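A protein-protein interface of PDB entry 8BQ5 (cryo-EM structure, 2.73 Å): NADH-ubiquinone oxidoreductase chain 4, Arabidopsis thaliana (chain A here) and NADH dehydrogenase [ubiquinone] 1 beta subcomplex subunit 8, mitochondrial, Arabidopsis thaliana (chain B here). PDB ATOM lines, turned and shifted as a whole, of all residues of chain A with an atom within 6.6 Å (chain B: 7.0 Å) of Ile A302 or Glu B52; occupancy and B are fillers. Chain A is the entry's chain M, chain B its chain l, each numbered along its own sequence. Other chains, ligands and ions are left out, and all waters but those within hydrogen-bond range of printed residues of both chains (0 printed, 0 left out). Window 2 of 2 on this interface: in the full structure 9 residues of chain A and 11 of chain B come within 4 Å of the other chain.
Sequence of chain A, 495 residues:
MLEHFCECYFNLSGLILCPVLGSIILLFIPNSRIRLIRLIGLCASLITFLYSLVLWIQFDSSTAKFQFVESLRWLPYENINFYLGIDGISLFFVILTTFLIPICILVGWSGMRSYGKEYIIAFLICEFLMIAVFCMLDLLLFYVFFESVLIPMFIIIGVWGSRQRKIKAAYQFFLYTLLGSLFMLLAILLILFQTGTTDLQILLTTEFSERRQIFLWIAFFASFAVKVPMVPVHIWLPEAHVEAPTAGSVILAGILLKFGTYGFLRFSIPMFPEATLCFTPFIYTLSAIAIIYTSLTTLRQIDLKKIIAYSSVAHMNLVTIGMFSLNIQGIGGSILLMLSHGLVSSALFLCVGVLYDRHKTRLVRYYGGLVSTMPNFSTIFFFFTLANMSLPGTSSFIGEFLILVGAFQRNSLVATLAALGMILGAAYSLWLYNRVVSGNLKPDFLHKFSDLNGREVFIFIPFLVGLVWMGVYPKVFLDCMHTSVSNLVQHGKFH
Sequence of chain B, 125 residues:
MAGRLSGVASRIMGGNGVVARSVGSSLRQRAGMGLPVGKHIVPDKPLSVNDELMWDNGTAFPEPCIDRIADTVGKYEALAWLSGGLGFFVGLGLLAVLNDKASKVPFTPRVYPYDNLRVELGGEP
Hydrophobic or aromatic side chains of chain A within 4 Å of the printed part of chain B: Ile A302 and Trp A431. Of the 7 printed residues of chain B, 5 touch a printed residue of chain A. Hydrophobic or aromatic side chains of chain B within 4 Å of the printed part of chain A: Leu B53.
The guanidinium group of Arg A300 lies within salt-bridge range of the side-chain carboxylate of Glu B52 (2.8 Å). The guanidinium group (NH1) of Arg A365 lies within salt-bridge range of the side-chain carboxylate (OD2) of Asp B51.
The backbone carbonyl oxygen (O) of Ile A302 is in hydrogen-bond range of the backbone NH (N) of Val A364, at 3.1 Å. The guanidinium group (NE) of Arg A435 lies within hydrogen-bond range of the backbone carbonyl oxygen (O) of Trp A431 (3.0 Å). N of Asn B50 sits at hydrogen-bond distance from OG of Ser B48 (3.3 Å).
Of chain B, only Glu B52 comes within 4 Å of Ile A302. Of chain A, only Arg A300 (2.8 Å), Ile A302 (3.8 Å) and Trp A431 (3.3 Å) come within 4 Å of Glu B52. Of the printed residues of chain A, Leu B53 touches Arg A300 (3.7 Å). Printed residues of chain A within 4 Å of Asn B50: Arg A300. Of the printed residues of chain A, Asp B51 touches Arg A365. Of the printed residues of chain B, Trp A431 touches Glu B52. Leu A299 touches none of the printed residues of chain B. Arg A435 touches none of the printed residues of chain B. The nearest residue of chain A that does not touch Glu B52 is Arg A435 (4.6 Å).
Among the printed residues, merely in contact across the chains: Arg A300 with Val B49 (3.98 Å), Arg A300 with Asn B50 (3.5 Å), Arg A300 with Leu B53 (3.7 Å), Ile A302 with Glu B52 (3.8 Å) and Trp A431 with Glu B52 (3.3 Å).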
ATOM      1  N   THR A 298     -19.896  20.163 -19.316  1.00  0.00           N
ATOM      2  CA  THR A 298     -18.749  19.895 -20.181  1.00  0.00           C
ATOM      3  C   THR A 298     -17.459  20.411 -19.559  1.00  0.00           C
ATOM      4  O   THR A 298     -16.401  19.784 -19.678  1.00  0.00           O
ATOM      5  CB  THR A 298     -18.971  20.533 -21.555  1.00  0.00           C
ATOM      6  OG1 THR A 298     -20.321  20.308 -21.980  1.00  0.00           O
ATOM      7  CG2 THR A 298     -18.020  19.945 -22.576  1.00  0.00           C
ATOM      8  N   LEU A 299     -17.536  21.562 -18.885  1.00  0.00           N
ATOM      9  CA  LEU A 299     -16.370  22.151 -18.235  1.00  0.00           C
ATOM     10  C   LEU A 299     -15.705  21.195 -17.255  1.00  0.00           C
ATOM     11  O   LEU A 299     -14.474  21.172 -17.151  1.00  0.00           O
ATOM     12  CB  LEU A 299     -16.783  23.429 -17.501  1.00  0.00           C
ATOM     13  CG  LEU A 299     -15.851  24.641 -17.448  1.00  0.00           C
ATOM     14  CD1 LEU A 299     -15.040  24.800 -18.718  1.00  0.00           C
ATOM     15  CD2 LEU A 299     -16.657  25.895 -17.163  1.00  0.00           C
ATOM     16  N   ARG A 300     -16.493  20.404 -16.528  1.00  0.00           N
ATOM     17  CA  ARG A 300     -15.982  19.584 -15.438  1.00  0.00           C
ATOM     18  C   ARG A 300     -15.744  18.132 -15.838  1.00  0.00           C
ATOM     19  O   ARG A 300     -15.427  17.308 -14.974  1.00  0.00           O
ATOM     20  CB  ARG A 300     -16.934  19.653 -14.244  1.00  0.00           C
ATOM     21  CG  ARG A 300     -17.046  21.040 -13.620  1.00  0.00           C
ATOM     22  CD  ARG A 300     -15.679  21.596 -13.242  1.00  0.00           C
ATOM     23  NE  ARG A 300     -14.992  20.753 -12.271  1.00  0.00           N
ATOM     24  CZ  ARG A 300     -15.229  20.762 -10.967  1.00  0.00           C
ATOM     25  NH1 ARG A 300     -16.118  21.580 -10.430  1.00  0.00           N
ATOM     26  NH2 ARG A 300     -14.556  19.927 -10.181  1.00  0.00           N
ATOM     27  N   GLN A 301     -15.891  17.792 -17.114  1.00  0.00           N
ATOM     28  CA  GLN A 301     -15.588  16.449 -17.584  1.00  0.00           C
ATOM     29  C   GLN A 301     -14.080  16.265 -17.695  1.00  0.00           C
ATOM     30  O   GLN A 301     -13.352  17.198 -18.045  1.00  0.00           O
ATOM     31  CB  GLN A 301     -16.258  16.185 -18.932  1.00  0.00           C
ATOM     32  CG  GLN A 301     -17.774  16.273 -18.894  1.00  0.00           C
ATOM     33  CD  GLN A 301     -18.397  15.217 -18.004  1.00  0.00           C
ATOM     34  OE1 GLN A 301     -18.108  14.029 -18.139  1.00  0.00           O
ATOM     35  NE2 GLN A 301     -19.254  15.647 -17.086  1.00  0.00           N
ATOM     36  N   ILE A 302     -13.614  15.056 -17.386  1.00  0.00           N
ATOM     37  CA  ILE A 302     -12.190  14.741 -17.348  1.00  0.00           C
ATOM     38  C   ILE A 302     -11.774  13.801 -18.460  1.00  0.00           C
ATOM     39  O   ILE A 302     -10.587  13.462 -18.563  1.00  0.00           O
ATOM     40  CB  ILE A 302     -11.789  14.158 -15.982  1.00  0.00           C
ATOM     41  CG1 ILE A 302     -12.471  12.804 -15.765  1.00  0.00           C
ATOM     42  CG2 ILE A 302     -12.156  15.123 -14.875  1.00  0.00           C
ATOM     43  CD1 ILE A 302     -12.205  12.196 -14.413  1.00  0.00           C
ATOM     44  N   ASP A 303     -12.710  13.367 -19.293  1.00  0.00           N
ATOM     45  CA  ASP A 303     -12.453  12.439 -20.380  1.00  0.00           C
ATOM     46  C   ASP A 303     -12.502  13.207 -21.693  1.00  0.00           C
ATOM     47  O   ASP A 303     -13.430  13.991 -21.921  1.00  0.00           O
ATOM     48  CB  ASP A 303     -13.479  11.300 -20.351  1.00  0.00           C
ATOM     49  CG  ASP A 303     -13.366  10.356 -21.537  1.00  0.00           C
ATOM     50  OD1 ASP A 303     -12.444  10.512 -22.356  1.00  0.00           O
ATOM     51  OD2 ASP A 303     -14.214   9.447 -21.649  1.00  0.00           O
ATOM     52  N   LEU A 304     -11.497  12.982 -22.544  1.00  0.00           N
ATOM     53  CA  LEU A 304     -11.424  13.652 -23.840  1.00  0.00           C
ATOM     54  C   LEU A 304     -12.710  13.470 -24.635  1.00  0.00           C
ATOM     55  O   LEU A 304     -13.289  14.434 -25.144  1.00  0.00           O
ATOM     56  CB  LEU A 304     -10.235  13.109 -24.634  1.00  0.00           C
ATOM     57  CG  LEU A 304      -8.857  13.724 -24.418  1.00  0.00           C
ATOM     58  CD1 LEU A 304      -7.782  12.760 -24.871  1.00  0.00           C
ATOM     59  CD2 LEU A 304      -8.762  15.007 -25.201  1.00  0.00           C
ATOM     60  N   LYS A 306     -15.643  12.399 -23.514  1.00  0.00           N
ATOM     61  CA  LYS A 306     -16.820  12.878 -22.795  1.00  0.00           C
ATOM     62  C   LYS A 306     -17.014  14.375 -22.998  1.00  0.00           C
ATOM     63  O   LYS A 306     -18.150  14.861 -23.028  1.00  0.00           O
ATOM     64  CB  LYS A 306     -16.707  12.554 -21.307  1.00  0.00           C
ATOM     65  CG  LYS A 306     -17.194  11.169 -20.942  1.00  0.00           C
ATOM     66  CD  LYS A 306     -18.671  11.181 -20.614  1.00  0.00           C
ATOM     67  CE  LYS A 306     -19.209   9.772 -20.435  1.00  0.00           C
ATOM     68  NZ  LYS A 306     -18.188   8.855 -19.853  1.00  0.00           N
ATOM     69  N   ILE A 307     -15.917  15.122 -23.121  1.00  0.00           N
ATOM     70  CA  ILE A 307     -16.021  16.557 -23.362  1.00  0.00           C
ATOM     71  C   ILE A 307     -16.588  16.827 -24.749  1.00  0.00           C
ATOM     72  O   ILE A 307     -17.525  17.617 -24.912  1.00  0.00           O
ATOM     73  CB  ILE A 307     -14.650  17.231 -23.171  1.00  0.00           C
ATOM     74  CG1 ILE A 307     -14.251  17.205 -21.696  1.00  0.00           C
ATOM     75  CG2 ILE A 307     -14.676  18.658 -23.699  1.00  0.00           C
ATOM     76  CD1 ILE A 307     -12.766  17.164 -21.464  1.00  0.00           C
ATOM     77  N   ARG A 362      -7.967   8.010 -22.492  1.00  0.00           N
ATOM     78  CA  ARG A 362      -8.847   9.128 -22.767  1.00  0.00           C
ATOM     79  C   ARG A 362      -8.810  10.171 -21.664  1.00  0.00           C
ATOM     80  O   ARG A 362      -9.391  11.249 -21.825  1.00  0.00           O
ATOM     81  CB  ARG A 362     -10.270   8.609 -22.967  1.00  0.00           C
ATOM     82  CG  ARG A 362     -10.569   8.101 -24.363  1.00  0.00           C
ATOM     83  CD  ARG A 362     -11.507   6.924 -24.286  1.00  0.00           C
ATOM     84  NE  ARG A 362     -12.622   7.171 -23.383  1.00  0.00           N
ATOM     85  CZ  ARG A 362     -13.577   6.291 -23.124  1.00  0.00           C
ATOM     86  NH1 ARG A 362     -13.620   5.118 -23.733  1.00  0.00           N
ATOM     87  NH2 ARG A 362     -14.485   6.572 -22.194  1.00  0.00           N
ATOM     88  N   LEU A 363      -8.137   9.878 -20.554  1.00  0.00           N
ATOM     89  CA  LEU A 363      -8.038  10.805 -19.437  1.00  0.00           C
ATOM     90  C   LEU A 363      -7.163  11.988 -19.832  1.00  0.00           C
ATOM     91  O   LEU A 363      -6.061  11.806 -20.358  1.00  0.00           O
ATOM     92  CB  LEU A 363      -7.470  10.091 -18.213  1.00  0.00           C
ATOM     93  CG  LEU A 363      -8.426   9.082 -17.574  1.00  0.00           C
ATOM     94  CD1 LEU A 363      -7.865   8.525 -16.276  1.00  0.00           C
ATOM     95  CD2 LEU A 363      -9.786   9.716 -17.342  1.00  0.00           C
ATOM     96  N   VAL A 364      -7.660  13.198 -19.572  1.00  0.00           N
ATOM     97  CA  VAL A 364      -6.947  14.410 -19.961  1.00  0.00           C
ATOM     98  C   VAL A 364      -5.639  14.545 -19.192  1.00  0.00           C
ATOM     99  O   VAL A 364      -4.633  15.011 -19.740  1.00  0.00           O
ATOM    100  CB  VAL A 364      -7.864  15.636 -19.761  1.00  0.00           C
ATOM    101  CG1 VAL A 364      -7.113  16.925 -20.009  1.00  0.00           C
ATOM    102  CG2 VAL A 364      -9.072  15.543 -20.676  1.00  0.00           C
ATOM    103  N   ARG A 365      -5.619  14.122 -17.927  1.00  0.00           N
ATOM    104  CA  ARG A 365      -4.452  14.357 -17.082  1.00  0.00           C
ATOM    105  C   ARG A 365      -3.216  13.614 -17.577  1.00  0.00           C
ATOM    106  O   ARG A 365      -2.089  14.019 -17.273  1.00  0.00           O
ATOM    107  CB  ARG A 365      -4.760  13.963 -15.638  1.00  0.00           C
ATOM    108  CG  ARG A 365      -3.600  14.202 -14.694  1.00  0.00           C
ATOM    109  CD  ARG A 365      -3.956  13.871 -13.260  1.00  0.00           C
ATOM    110  NE  ARG A 365      -2.828  14.133 -12.372  1.00  0.00           N
ATOM    111  CZ  ARG A 365      -2.898  14.121 -11.048  1.00  0.00           C
ATOM    112  NH1 ARG A 365      -4.029  13.849 -10.418  1.00  0.00           N
ATOM    113  NH2 ARG A 365      -1.806  14.394 -10.340  1.00  0.00           N
ATOM    114  N   TRP A 431      -9.841  25.193 -22.677  1.00  0.00           N
ATOM    115  CA  TRP A 431      -9.306  24.418 -21.562  1.00  0.00           C
ATOM    116  C   TRP A 431      -8.897  23.024 -22.014  1.00  0.00           C
ATOM    117  O   TRP A 431      -7.844  22.514 -21.616  1.00  0.00           O
ATOM    118  CB  TRP A 431     -10.326  24.329 -20.428  1.00  0.00           C
ATOM    119  CG  TRP A 431      -9.674  24.136 -19.096  1.00  0.00           C
ATOM    120  CD1 TRP A 431      -8.363  24.350 -18.792  1.00  0.00           C
ATOM    121  CD2 TRP A 431     -10.289  23.652 -17.895  1.00  0.00           C
ATOM    122  NE1 TRP A 431      -8.125  24.049 -17.476  1.00  0.00           N
ATOM    123  CE2 TRP A 431      -9.290  23.616 -16.902  1.00  0.00           C
ATOM    124  CE3 TRP A 431     -11.586  23.252 -17.561  1.00  0.00           C
ATOM    125  CZ2 TRP A 431      -9.548  23.198 -15.598  1.00  0.00           C
ATOM    126  CZ3 TRP A 431     -11.839  22.837 -16.266  1.00  0.00           C
ATOM    127  CH2 TRP A 431     -10.826  22.813 -15.300  1.00  0.00           C
ATOM    128  N   ARG A 435      -4.863  21.794 -21.962  1.00  0.00           N
ATOM    129  CA  ARG A 435      -4.482  20.715 -21.059  1.00  0.00           C
ATOM    130  C   ARG A 435      -3.908  19.522 -21.816  1.00  0.00           C
ATOM    131  O   ARG A 435      -3.144  18.738 -21.245  1.00  0.00           O
ATOM    132  CB  ARG A 435      -5.683  20.287 -20.217  1.00  0.00           C
ATOM    133  CG  ARG A 435      -6.049  21.275 -19.122  1.00  0.00           C
ATOM    134  CD  ARG A 435      -7.291  20.832 -18.374  1.00  0.00           C
ATOM    135  NE  ARG A 435      -8.447  20.737 -19.255  1.00  0.00           N
ATOM    136  CZ  ARG A 435      -9.690  20.529 -18.841  1.00  0.00           C
ATOM    137  NH1 ARG A 435      -9.977  20.396 -17.558  1.00  0.00           N
ATOM    138  NH2 ARG A 435     -10.667  20.454 -19.739  1.00  0.00           N
ATOM    139  N   SER B  48      -8.644  14.079  -5.213  1.00  0.00           N
ATOM    140  CA  SER B  48      -9.927  14.629  -4.816  1.00  0.00           C
ATOM    141  C   SER B  48     -10.830  14.797  -6.034  1.00  0.00           C
ATOM    142  O   SER B  48     -10.394  14.720  -7.185  1.00  0.00           O
ATOM    143  CB  SER B  48      -9.742  15.965  -4.101  1.00  0.00           C
ATOM    144  OG  SER B  48     -10.921  16.745  -4.179  1.00  0.00           O
ATOM    145  N   VAL B  49     -12.117  15.017  -5.768  1.00  0.00           N
ATOM    146  CA  VAL B  49     -13.075  15.154  -6.859  1.00  0.00           C
ATOM    147  C   VAL B  49     -12.880  16.477  -7.597  1.00  0.00           C
ATOM    148  O   VAL B  49     -12.974  16.531  -8.828  1.00  0.00           O
ATOM    149  CB  VAL B  49     -14.511  14.967  -6.332  1.00  0.00           C
ATOM    150  CG1 VAL B  49     -14.598  13.666  -5.553  1.00  0.00           C
ATOM    151  CG2 VAL B  49     -14.924  16.117  -5.439  1.00  0.00           C
ATOM    152  N   ASN B  50     -12.591  17.557  -6.870  1.00  0.00           N
ATOM    153  CA  ASN B  50     -12.295  18.850  -7.492  1.00  0.00           C
ATOM    154  C   ASN B  50     -10.784  19.024  -7.632  1.00  0.00           C
ATOM    155  O   ASN B  50     -10.183  19.982  -7.144  1.00  0.00           O
ATOM    156  CB  ASN B  50     -12.914  19.992  -6.687  1.00  0.00           C
ATOM    157  CG  ASN B  50     -14.430  19.978  -6.713  1.00  0.00           C
ATOM    158  OD1 ASN B  50     -15.053  18.921  -6.726  1.00  0.00           O
ATOM    159  ND2 ASN B  50     -15.030  21.163  -6.721  1.00  0.00           N
ATOM    160  N   ASP B  51     -10.170  18.066  -8.324  1.00  0.00           N
ATOM    161  CA  ASP B  51      -8.736  18.088  -8.565  1.00  0.00           C
ATOM    162  C   ASP B  51      -8.402  18.657  -9.941  1.00  0.00           C
ATOM    163  O   ASP B  51      -7.294  19.165 -10.141  1.00  0.00           O
ATOM    164  CB  ASP B  51      -8.176  16.660  -8.406  1.00  0.00           C
ATOM    165  CG  ASP B  51      -6.674  16.546  -8.666  1.00  0.00           C
ATOM    166  OD1 ASP B  51      -5.978  17.538  -8.937  1.00  0.00           O
ATOM    167  OD2 ASP B  51      -6.164  15.418  -8.573  1.00  0.00           O
ATOM    168  N   GLU B  52      -9.351  18.645 -10.878  1.00  0.00           N
ATOM    169  CA  GLU B  52      -9.075  19.144 -12.219  1.00  0.00           C
ATOM    170  C   GLU B  52      -8.934  20.661 -12.265  1.00  0.00           C
ATOM    171  O   GLU B  52      -8.453  21.193 -13.270  1.00  0.00           O
ATOM    172  CB  GLU B  52     -10.181  18.697 -13.174  1.00  0.00           C
ATOM    173  CG  GLU B  52     -11.493  19.443 -12.989  1.00  0.00           C
ATOM    174  CD  GLU B  52     -12.578  18.577 -12.383  1.00  0.00           C
ATOM    175  OE1 GLU B  52     -13.506  18.179 -13.116  1.00  0.00           O
ATOM    176  OE2 GLU B  52     -12.502  18.296 -11.169  1.00  0.00           O
ATOM    177  N   LEU B  53      -9.336  21.367 -11.207  1.00  0.00           N
ATOM    178  CA  LEU B  53      -9.327  22.823 -11.200  1.00  0.00           C
ATOM    179  C   LEU B  53      -8.287  23.434 -10.270  1.00  0.00           C
ATOM    180  O   LEU B  53      -7.875  24.577 -10.501  1.00  0.00           O
ATOM    181  CB  LEU B  53     -10.725  23.362 -10.849  1.00  0.00           C
ATOM    182  CG  LEU B  53     -11.556  22.829  -9.671  1.00  0.00           C
ATOM    183  CD1 LEU B  53     -10.944  23.126  -8.312  1.00  0.00           C
ATOM    184  CD2 LEU B  53     -12.963  23.393  -9.742  1.00  0.00           C
ATOM    185  N   MET B  54      -7.847  22.720  -9.239  1.00  0.00           N
ATOM    186  CA  MET B  54      -6.881  23.274  -8.291  1.00  0.00           C
ATOM    187  C   MET B  54      -5.461  23.244  -8.846  1.00  0.00           C
ATOM    188  O   MET B  54      -4.570  23.916  -8.323  1.00  0.00           O
ATOM    189  CB  MET B  54      -6.937  22.517  -6.961  1.00  0.00           C
ATOM    190  CG  MET B  54      -8.097  22.915  -6.061  1.00  0.00           C
ATOM    191  SD  MET B  54      -7.697  24.273  -4.940  1.00  0.00           S
ATOM    192  CE  MET B  54      -5.928  24.062  -4.760  1.00  0.00           C
